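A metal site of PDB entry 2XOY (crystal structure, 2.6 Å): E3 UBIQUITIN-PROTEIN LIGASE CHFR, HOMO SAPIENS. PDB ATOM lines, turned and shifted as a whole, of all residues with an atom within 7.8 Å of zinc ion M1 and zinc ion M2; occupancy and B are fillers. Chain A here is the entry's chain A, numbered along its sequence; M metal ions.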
ATOM      1  N   ARG A  26     -37.031  -7.628  12.616  1.00  0.00           N
ATOM      2  CA  ARG A  26     -36.440  -7.806  13.946  1.00  0.00           C
ATOM      3  C   ARG A  26     -36.211  -6.505  14.730  1.00  0.00           C
ATOM      4  O   ARG A  26     -36.264  -6.502  15.959  1.00  0.00           O
ATOM      5  CB  ARG A  26     -35.113  -8.554  13.847  1.00  0.00           C
ATOM      6  CG  ARG A  26     -35.240 -10.048  13.620  1.00  0.00           C
ATOM      7  CD  ARG A  26     -33.930 -10.719  13.921  1.00  0.00           C
ATOM      8  NE  ARG A  26     -33.367 -11.403  12.767  1.00  0.00           N
ATOM      9  CZ  ARG A  26     -32.078 -11.713  12.630  1.00  0.00           C
ATOM     10  NH1 ARG A  26     -31.219 -11.368  13.587  1.00  0.00           N
ATOM     11  NH2 ARG A  26     -31.644 -12.338  11.544  1.00  0.00           N
ATOM     12  N   LEU A  81     -34.502  -6.653   1.480  1.00  0.00           N
ATOM     13  CA  LEU A  81     -34.598  -8.097   1.679  1.00  0.00           C
ATOM     14  C   LEU A  81     -33.258  -8.808   1.494  1.00  0.00           C
ATOM     15  O   LEU A  81     -32.645  -8.747   0.413  1.00  0.00           O
ATOM     16  CB  LEU A  81     -35.664  -8.706   0.769  1.00  0.00           C
ATOM     17  CG  LEU A  81     -37.129  -8.379   1.078  1.00  0.00           C
ATOM     18  CD1 LEU A  81     -38.059  -9.018   0.065  1.00  0.00           C
ATOM     19  CD2 LEU A  81     -37.504  -8.829   2.477  1.00  0.00           C
ATOM     20  N   CYS A  82     -32.803  -9.463   2.564  1.00  0.00           N
ATOM     21  CA  CYS A  82     -31.600 -10.278   2.480  1.00  0.00           C
ATOM     22  C   CYS A  82     -31.789 -11.198   1.303  1.00  0.00           C
ATOM     23  O   CYS A  82     -32.808 -11.862   1.198  1.00  0.00           O
ATOM     24  CB  CYS A  82     -31.354 -11.078   3.754  1.00  0.00           C
ATOM     25  SG  CYS A  82     -29.954 -12.208   3.623  1.00  0.00           S
ATOM     26  N   THR A  83     -30.819 -11.210   0.408  1.00  0.00           N
ATOM     27  CA  THR A  83     -30.894 -11.998  -0.805  1.00  0.00           C
ATOM     28  C   THR A  83     -30.858 -13.493  -0.499  1.00  0.00           C
ATOM     29  O   THR A  83     -31.291 -14.301  -1.307  1.00  0.00           O
ATOM     30  CB  THR A  83     -29.728 -11.640  -1.726  1.00  0.00           C
ATOM     31  OG1 THR A  83     -29.812 -10.244  -2.058  1.00  0.00           O
ATOM     32  CG2 THR A  83     -29.732 -12.512  -2.994  1.00  0.00           C
ATOM     33  N   CYS A  84     -30.339 -13.848   0.670  1.00  0.00           N
ATOM     34  CA  CYS A  84     -30.120 -15.250   0.996  1.00  0.00           C
ATOM     35  C   CYS A  84     -31.278 -15.796   1.791  1.00  0.00           C
ATOM     36  O   CYS A  84     -31.871 -16.809   1.422  1.00  0.00           O
ATOM     37  CB  CYS A  84     -28.803 -15.427   1.774  1.00  0.00           C
ATOM     38  SG  CYS A  84     -28.771 -16.899   2.858  1.00  0.00           S
ATOM     39  N   CYS A  85     -31.589 -15.131   2.889  1.00  0.00           N
ATOM     40  CA  CYS A  85     -32.575 -15.667   3.803  1.00  0.00           C
ATOM     41  C   CYS A  85     -33.982 -15.123   3.536  1.00  0.00           C
ATOM     42  O   CYS A  85     -34.957 -15.632   4.097  1.00  0.00           O
ATOM     43  CB  CYS A  85     -32.154 -15.404   5.247  1.00  0.00           C
ATOM     44  SG  CYS A  85     -32.396 -13.708   5.796  1.00  0.00           S
ATOM     45  N   PHE A  86     -34.083 -14.108   2.685  1.00  0.00           N
ATOM     46  CA  PHE A  86     -35.366 -13.550   2.241  1.00  0.00           C
ATOM     47  C   PHE A  86     -36.083 -12.640   3.255  1.00  0.00           C
ATOM     48  O   PHE A  86     -37.103 -12.032   2.928  1.00  0.00           O
ATOM     49  CB  PHE A  86     -36.320 -14.664   1.809  1.00  0.00           C
ATOM     50  CG  PHE A  86     -35.805 -15.504   0.672  1.00  0.00           C
ATOM     51  CD1 PHE A  86     -35.223 -14.900  -0.441  1.00  0.00           C
ATOM     52  CD2 PHE A  86     -35.898 -16.889   0.705  1.00  0.00           C
ATOM     53  CE1 PHE A  86     -34.760 -15.669  -1.494  1.00  0.00           C
ATOM     54  CE2 PHE A  86     -35.435 -17.658  -0.348  1.00  0.00           C
ATOM     55  CZ  PHE A  86     -34.854 -17.049  -1.447  1.00  0.00           C
ATOM     56  N   GLN A  87     -35.549 -12.537   4.461  1.00  0.00           N
ATOM     57  CA  GLN A  87     -36.125 -11.686   5.493  1.00  0.00           C
ATOM     58  C   GLN A  87     -35.738 -10.213   5.304  1.00  0.00           C
ATOM     59  O   GLN A  87     -34.734  -9.900   4.659  1.00  0.00           O
ATOM     60  CB  GLN A  87     -35.688 -12.158   6.877  1.00  0.00           C
ATOM     61  CG  GLN A  87     -35.887 -13.650   7.105  1.00  0.00           C
ATOM     62  CD  GLN A  87     -37.342 -14.085   6.978  1.00  0.00           C
ATOM     63  OE1 GLN A  87     -38.177 -13.749   7.829  1.00  0.00           O
ATOM     64  NE2 GLN A  87     -37.650 -14.833   5.926  1.00  0.00           N
ATOM     65  N   PRO A  88     -36.550  -9.308   5.872  1.00  0.00           N
ATOM     66  CA  PRO A  88     -36.344  -7.848   5.844  1.00  0.00           C
ATOM     67  C   PRO A  88     -35.384  -7.310   6.901  1.00  0.00           C
ATOM     68  O   PRO A  88     -35.405  -7.733   8.056  1.00  0.00           O
ATOM     69  CB  PRO A  88     -37.735  -7.307   6.142  1.00  0.00           C
ATOM     70  CG  PRO A  88     -38.357  -8.367   6.978  1.00  0.00           C
ATOM     71  CD  PRO A  88     -37.885  -9.653   6.385  1.00  0.00           C
ATOM     72  N   MET A  89     -34.542  -6.369   6.482  1.00  0.00           N
ATOM     73  CA  MET A  89     -33.697  -5.592   7.387  1.00  0.00           C
ATOM     74  C   MET A  89     -33.873  -4.127   7.018  1.00  0.00           C
ATOM     75  O   MET A  89     -34.279  -3.806   5.895  1.00  0.00           O
ATOM     76  CB  MET A  89     -32.235  -5.983   7.231  1.00  0.00           C
ATOM     77  CG  MET A  89     -31.688  -5.694   5.848  1.00  0.00           C
ATOM     78  SD  MET A  89     -30.070  -6.441   5.570  1.00  0.00           S
ATOM     79  CE  MET A  89     -29.808  -6.046   3.840  1.00  0.00           C
ATOM     80  N   PRO A 113     -28.160  -7.166  -1.570  1.00  0.00           N
ATOM     81  CA  PRO A 113     -28.128  -6.977  -0.115  1.00  0.00           C
ATOM     82  C   PRO A 113     -28.185  -8.293   0.661  1.00  0.00           C
ATOM     83  O   PRO A 113     -28.845  -9.250   0.229  1.00  0.00           O
ATOM     84  CB  PRO A 113     -29.423  -6.182   0.148  1.00  0.00           C
ATOM     85  CG  PRO A 113     -30.168  -6.158  -1.182  1.00  0.00           C
ATOM     86  CD  PRO A 113     -29.537  -7.169  -2.059  1.00  0.00           C
ATOM     87  N   PHE A 114     -27.507  -8.312   1.812  1.00  0.00           N
ATOM     88  CA  PHE A 114     -27.414  -9.518   2.632  1.00  0.00           C
ATOM     89  C   PHE A 114     -27.358  -9.129   4.083  1.00  0.00           C
ATOM     90  O   PHE A 114     -26.725  -8.139   4.431  1.00  0.00           O
ATOM     91  CB  PHE A 114     -26.143 -10.299   2.270  1.00  0.00           C
ATOM     92  CG  PHE A 114     -26.159 -10.877   0.879  1.00  0.00           C
ATOM     93  CD1 PHE A 114     -26.604 -12.173   0.665  1.00  0.00           C
ATOM     94  CD2 PHE A 114     -25.738 -10.130  -0.204  1.00  0.00           C
ATOM     95  CE1 PHE A 114     -26.617 -12.723  -0.592  1.00  0.00           C
ATOM     96  CE2 PHE A 114     -25.747 -10.677  -1.470  1.00  0.00           C
ATOM     97  CZ  PHE A 114     -26.192 -11.983  -1.663  1.00  0.00           C
ATOM     98  N   CYS A 115     -27.986  -9.913   4.943  1.00  0.00           N
ATOM     99  CA  CYS A 115     -28.170  -9.517   6.339  1.00  0.00           C
ATOM    100  C   CYS A 115     -27.047  -9.958   7.249  1.00  0.00           C
ATOM    101  O   CYS A 115     -26.892  -9.429   8.352  1.00  0.00           O
ATOM    102  CB  CYS A 115     -29.512 -10.002   6.890  1.00  0.00           C
ATOM    103  SG  CYS A 115     -29.585 -11.759   7.383  1.00  0.00           S
ATOM    104  N   HIS A 116     -26.254 -10.928   6.802  1.00  0.00           N
ATOM    105  CA  HIS A 116     -25.424 -11.656   7.748  1.00  0.00           C
ATOM    106  C   HIS A 116     -24.475 -10.795   8.578  1.00  0.00           C
ATOM    107  O   HIS A 116     -24.368 -10.974   9.778  1.00  0.00           O
ATOM    108  CB  HIS A 116     -24.624 -12.740   7.058  1.00  0.00           C
ATOM    109  CG  HIS A 116     -23.932 -13.654   8.002  1.00  0.00           C
ATOM    110  ND1 HIS A 116     -24.617 -14.587   8.750  1.00  0.00           N
ATOM    111  CD2 HIS A 116     -22.631 -13.765   8.356  1.00  0.00           C
ATOM    112  CE1 HIS A 116     -23.759 -15.245   9.510  1.00  0.00           C
ATOM    113  NE2 HIS A 116     -22.542 -14.764   9.285  1.00  0.00           N
ATOM    114  N   LEU A 117     -23.799  -9.864   7.939  1.00  0.00           N
ATOM    115  CA  LEU A 117     -22.878  -9.003   8.653  1.00  0.00           C
ATOM    116  C   LEU A 117     -23.611  -7.978   9.485  1.00  0.00           C
ATOM    117  O   LEU A 117     -23.105  -7.534  10.516  1.00  0.00           O
ATOM    118  CB  LEU A 117     -21.916  -8.305   7.691  1.00  0.00           C
ATOM    119  CG  LEU A 117     -20.690  -9.116   7.288  1.00  0.00           C
ATOM    120  CD1 LEU A 117     -19.865  -8.341   6.292  1.00  0.00           C
ATOM    121  CD2 LEU A 117     -19.858  -9.489   8.533  1.00  0.00           C
ATOM    122  N   TRP A 119     -26.733  -8.283  11.193  1.00  0.00           N
ATOM    123  CA  TRP A 119     -27.270  -8.876  12.431  1.00  0.00           C
ATOM    124  C   TRP A 119     -27.314 -10.403  12.474  1.00  0.00           C
ATOM    125  O   TRP A 119     -28.023 -10.969  13.307  1.00  0.00           O
ATOM    126  CB  TRP A 119     -28.668  -8.323  12.741  1.00  0.00           C
ATOM    127  CG  TRP A 119     -29.722  -8.645  11.696  1.00  0.00           C
ATOM    128  CD1 TRP A 119     -29.635  -9.572  10.706  1.00  0.00           C
ATOM    129  CD2 TRP A 119     -31.014  -8.035  11.569  1.00  0.00           C
ATOM    130  NE1 TRP A 119     -30.793  -9.569   9.959  1.00  0.00           N
ATOM    131  CE2 TRP A 119     -31.657  -8.641  10.463  1.00  0.00           C
ATOM    132  CE3 TRP A 119     -31.706  -7.041  12.276  1.00  0.00           C
ATOM    133  CZ2 TRP A 119     -32.941  -8.273  10.049  1.00  0.00           C
ATOM    134  CZ3 TRP A 119     -32.973  -6.683  11.867  1.00  0.00           C
ATOM    135  CH2 TRP A 119     -33.584  -7.295  10.763  1.00  0.00           C
ATOM    136  N   GLY A 120     -26.600 -11.064  11.581  1.00  0.00           N
ATOM    137  CA  GLY A 120     -26.569 -12.531  11.550  1.00  0.00           C
ATOM    138  C   GLY A 120     -27.723 -13.194  10.812  1.00  0.00           C
ATOM    139  O   GLY A 120     -28.884 -13.128  11.220  1.00  0.00           O
ATOM    140  N   CYS A 121     -27.387 -13.860   9.713  1.00  0.00           N
ATOM    141  CA  CYS A 121     -28.374 -14.564   8.907  1.00  0.00           C
ATOM    142  C   CYS A 121     -28.583 -16.005   9.407  1.00  0.00           C
ATOM    143  O   CYS A 121     -27.710 -16.584  10.047  1.00  0.00           O
ATOM    144  CB  CYS A 121     -27.928 -14.583   7.452  1.00  0.00           C
ATOM    145  SG  CYS A 121     -29.061 -15.373   6.314  1.00  0.00           S
ATOM    146  N   THR A 122     -29.749 -16.572   9.098  1.00  0.00           N
ATOM    147  CA  THR A 122     -30.017 -17.977   9.419  1.00  0.00           C
ATOM    148  C   THR A 122     -30.920 -18.662   8.418  1.00  0.00           C
ATOM    149  O   THR A 122     -32.073 -18.269   8.210  1.00  0.00           O
ATOM    150  CB  THR A 122     -30.647 -18.143  10.817  1.00  0.00           C
ATOM    151  OG1 THR A 122     -29.614 -18.058  11.812  1.00  0.00           O
ATOM    152  CG2 THR A 122     -31.312 -19.513  10.923  1.00  0.00           C
ATOM    153  N   ARG A 123     -30.389 -19.706   7.804  1.00  0.00           N
ATOM    154  CA  ARG A 123     -31.127 -20.498   6.843  1.00  0.00           C
ATOM    155  C   ARG A 123     -30.322 -21.759   6.610  1.00  0.00           C
ATOM    156  O   ARG A 123     -29.090 -21.767   6.764  1.00  0.00           O
ATOM    157  CB  ARG A 123     -31.309 -19.727   5.535  1.00  0.00           C
ATOM    158  CG  ARG A 123     -32.196 -20.434   4.513  1.00  0.00           C
ATOM    159  CD  ARG A 123     -32.409 -19.591   3.267  1.00  0.00           C
ATOM    160  NE  ARG A 123     -31.172 -19.458   2.515  1.00  0.00           N
ATOM    161  CZ  ARG A 123     -30.871 -20.197   1.449  1.00  0.00           C
ATOM    162  NH1 ARG A 123     -31.714 -21.115   1.008  1.00  0.00           N
ATOM    163  NH2 ARG A 123     -29.711 -20.012   0.822  1.00  0.00           N
ATOM    164  N   GLY A 125     -28.250 -24.021   4.735  1.00  0.00           N
ATOM    165  CA  GLY A 125     -27.414 -23.877   3.555  1.00  0.00           C
ATOM    166  C   GLY A 125     -26.693 -22.553   3.577  1.00  0.00           C
ATOM    167  O   GLY A 125     -25.780 -22.312   2.779  1.00  0.00           O
ATOM    168  N   CYS A 126     -27.104 -21.677   4.490  1.00  0.00           N
ATOM    169  CA  CYS A 126     -26.399 -20.431   4.678  1.00  0.00           C
ATOM    170  C   CYS A 126     -25.234 -20.671   5.616  1.00  0.00           C
ATOM    171  O   CYS A 126     -25.424 -20.924   6.803  1.00  0.00           O
ATOM    172  CB  CYS A 126     -27.320 -19.326   5.236  1.00  0.00           C
ATOM    173  SG  CYS A 126     -26.421 -17.785   5.617  1.00  0.00           S
ATOM    174  N   TYR A 127     -24.020 -20.593   5.066  1.00  0.00           N
ATOM    175  CA  TYR A 127     -22.789 -20.792   5.831  1.00  0.00           C
ATOM    176  C   TYR A 127     -22.318 -19.507   6.521  1.00  0.00           C
ATOM    177  O   TYR A 127     -21.336 -19.529   7.270  1.00  0.00           O
ATOM    178  CB  TYR A 127     -21.699 -21.267   4.893  1.00  0.00           C
ATOM    179  CG  TYR A 127     -22.055 -22.461   4.031  1.00  0.00           C
ATOM    180  CD1 TYR A 127     -22.572 -23.618   4.584  1.00  0.00           C
ATOM    181  CD2 TYR A 127     -21.833 -22.442   2.661  1.00  0.00           C
ATOM    182  CE1 TYR A 127     -22.886 -24.714   3.802  1.00  0.00           C
ATOM    183  CE2 TYR A 127     -22.135 -23.520   1.879  1.00  0.00           C
ATOM    184  CZ  TYR A 127     -22.663 -24.652   2.443  1.00  0.00           C
ATOM    185  OH  TYR A 127     -22.969 -25.743   1.644  1.00  0.00           O
ATOM    186  N   GLY A 128     -23.018 -18.402   6.250  1.00  0.00           N
ATOM    187  CA  GLY A 128     -22.527 -17.049   6.523  1.00  0.00           C
ATOM    188  C   GLY A 128     -22.406 -16.302   5.194  1.00  0.00           C
ATOM    189  O   GLY A 128     -21.352 -16.295   4.561  1.00  0.00           O
ATOM    190  N   CYS A 129     -23.491 -15.669   4.763  1.00  0.00           N
ATOM    191  CA  CYS A 129     -23.602 -15.194   3.377  1.00  0.00           C
ATOM    192  C   CYS A 129     -22.879 -13.891   3.053  1.00  0.00           C
ATOM    193  O   CYS A 129     -22.970 -13.400   1.931  1.00  0.00           O
ATOM    194  CB  CYS A 129     -25.075 -15.113   2.944  1.00  0.00           C
ATOM    195  SG  CYS A 129     -26.194 -14.253   4.106  1.00  0.00           S
ATOM    196  N   LEU A 130     -22.174 -13.309   4.022  1.00  0.00           N
ATOM    197  CA  LEU A 130     -21.377 -12.111   3.752  1.00  0.00           C
ATOM    198  C   LEU A 130     -20.148 -12.039   4.644  1.00  0.00           C
ATOM    199  O   LEU A 130     -20.241 -12.172   5.863  1.00  0.00           O
ATOM    200  CB  LEU A 130     -22.222 -10.831   3.868  1.00  0.00           C
ATOM    201  CG  LEU A 130     -21.742  -9.566   3.144  1.00  0.00           C
ATOM    202  CD1 LEU A 130     -22.023  -9.633   1.636  1.00  0.00           C
ATOM    203  CD2 LEU A 130     -22.345  -8.282   3.753  1.00  0.00           C
ATOM    204  N   TYR A 199     -21.614 -15.205  -0.723  1.00  0.00           N
ATOM    205  CA  TYR A 199     -21.314 -16.596  -0.936  1.00  0.00           C
ATOM    206  C   TYR A 199     -21.093 -16.851  -2.425  1.00  0.00           C
ATOM    207  O   TYR A 199     -20.062 -17.423  -2.801  1.00  0.00           O
ATOM    208  CB  TYR A 199     -22.421 -17.513  -0.363  1.00  0.00           C
ATOM    209  CG  TYR A 199     -22.311 -18.932  -0.880  1.00  0.00           C
ATOM    210  CD1 TYR A 199     -21.326 -19.796  -0.431  1.00  0.00           C
ATOM    211  CD2 TYR A 199     -23.202 -19.413  -1.832  1.00  0.00           C
ATOM    212  CE1 TYR A 199     -21.222 -21.080  -0.915  1.00  0.00           C
ATOM    213  CE2 TYR A 199     -23.110 -20.700  -2.322  1.00  0.00           C
ATOM    214  CZ  TYR A 199     -22.112 -21.523  -1.868  1.00  0.00           C
ATOM    215  OH  TYR A 199     -22.012 -22.815  -2.355  1.00  0.00           O
HETATM  216 ZN    ZN M   1     -27.592 -15.946   4.551  1.00  0.00          ZN
HETATM  217 ZN    ZN M   2     -30.130 -13.055   5.708  1.00  0.00          ZN
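The side-chain sulfur (SG) of Cys 115 lies close to the indole nitrogen (NE1) of Trp 119 (3.6 Å). The backbone carbonyl oxygen (O) of Cys 129 is in hydrogen-bond range of the backbone NH (N) of Tyr 199 (3.5 Å). SG of Cys 82 lies close to N of Cys 84 (3.4 Å). The backbone carbonyl oxygen (O) of Gln 87 lies within hydrogen-bond range of the backbone NH (N) of Cys 82 (2.9 Å). The backbone carbonyl oxygen of Cys 84 lies within hydrogen-bond range of the guanidinium group of Arg 123, at 2.9 Å. The side-chain amide nitrogen (NE2) of Gln 87 is in hydrogen-bond range of the backbone carbonyl oxygen (O) of Cys 85 (3.4 Å). A ring nitrogen (ND1) of His 116 is in hydrogen-bond range of the backbone NH of Cys 121, 3.0 Å away. N of Gly 128 sits close to SG of Cys 126, at 3.5 Å.
Within 4 Å of zinc ion M1: Cys 84, Cys 121, Cys 126 and Cys 129. The nearest printed residue that does not touch zinc ion M1 is Cys 85 (4.4 Å).
Of the 27 residues printed, 4 come within 4 Å of zinc ion M2.
The side-chain sulfur (SG) of Cys 129 binds zinc ion M1 (2.2 Å). SG of Cys 84 is bound to zinc ion M1, 2.3 Å away. SG of Cys 121 is bound to zinc ion M1 (2.4 Å). SG of Cys 126 is bound to zinc ion M1 (2.4 Å).
Zinc ion M2 is bound by the side-chain sulfur (SG) of Cys 115 (2.2 Å), the side-chain sulfur (SG) of Cys 82 (2.3 Å), the side-chain sulfur (SG) of Cys 85 (2.4 Å) and the side-chain sulfur (SG) of Cys 121 (2.6 Å).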
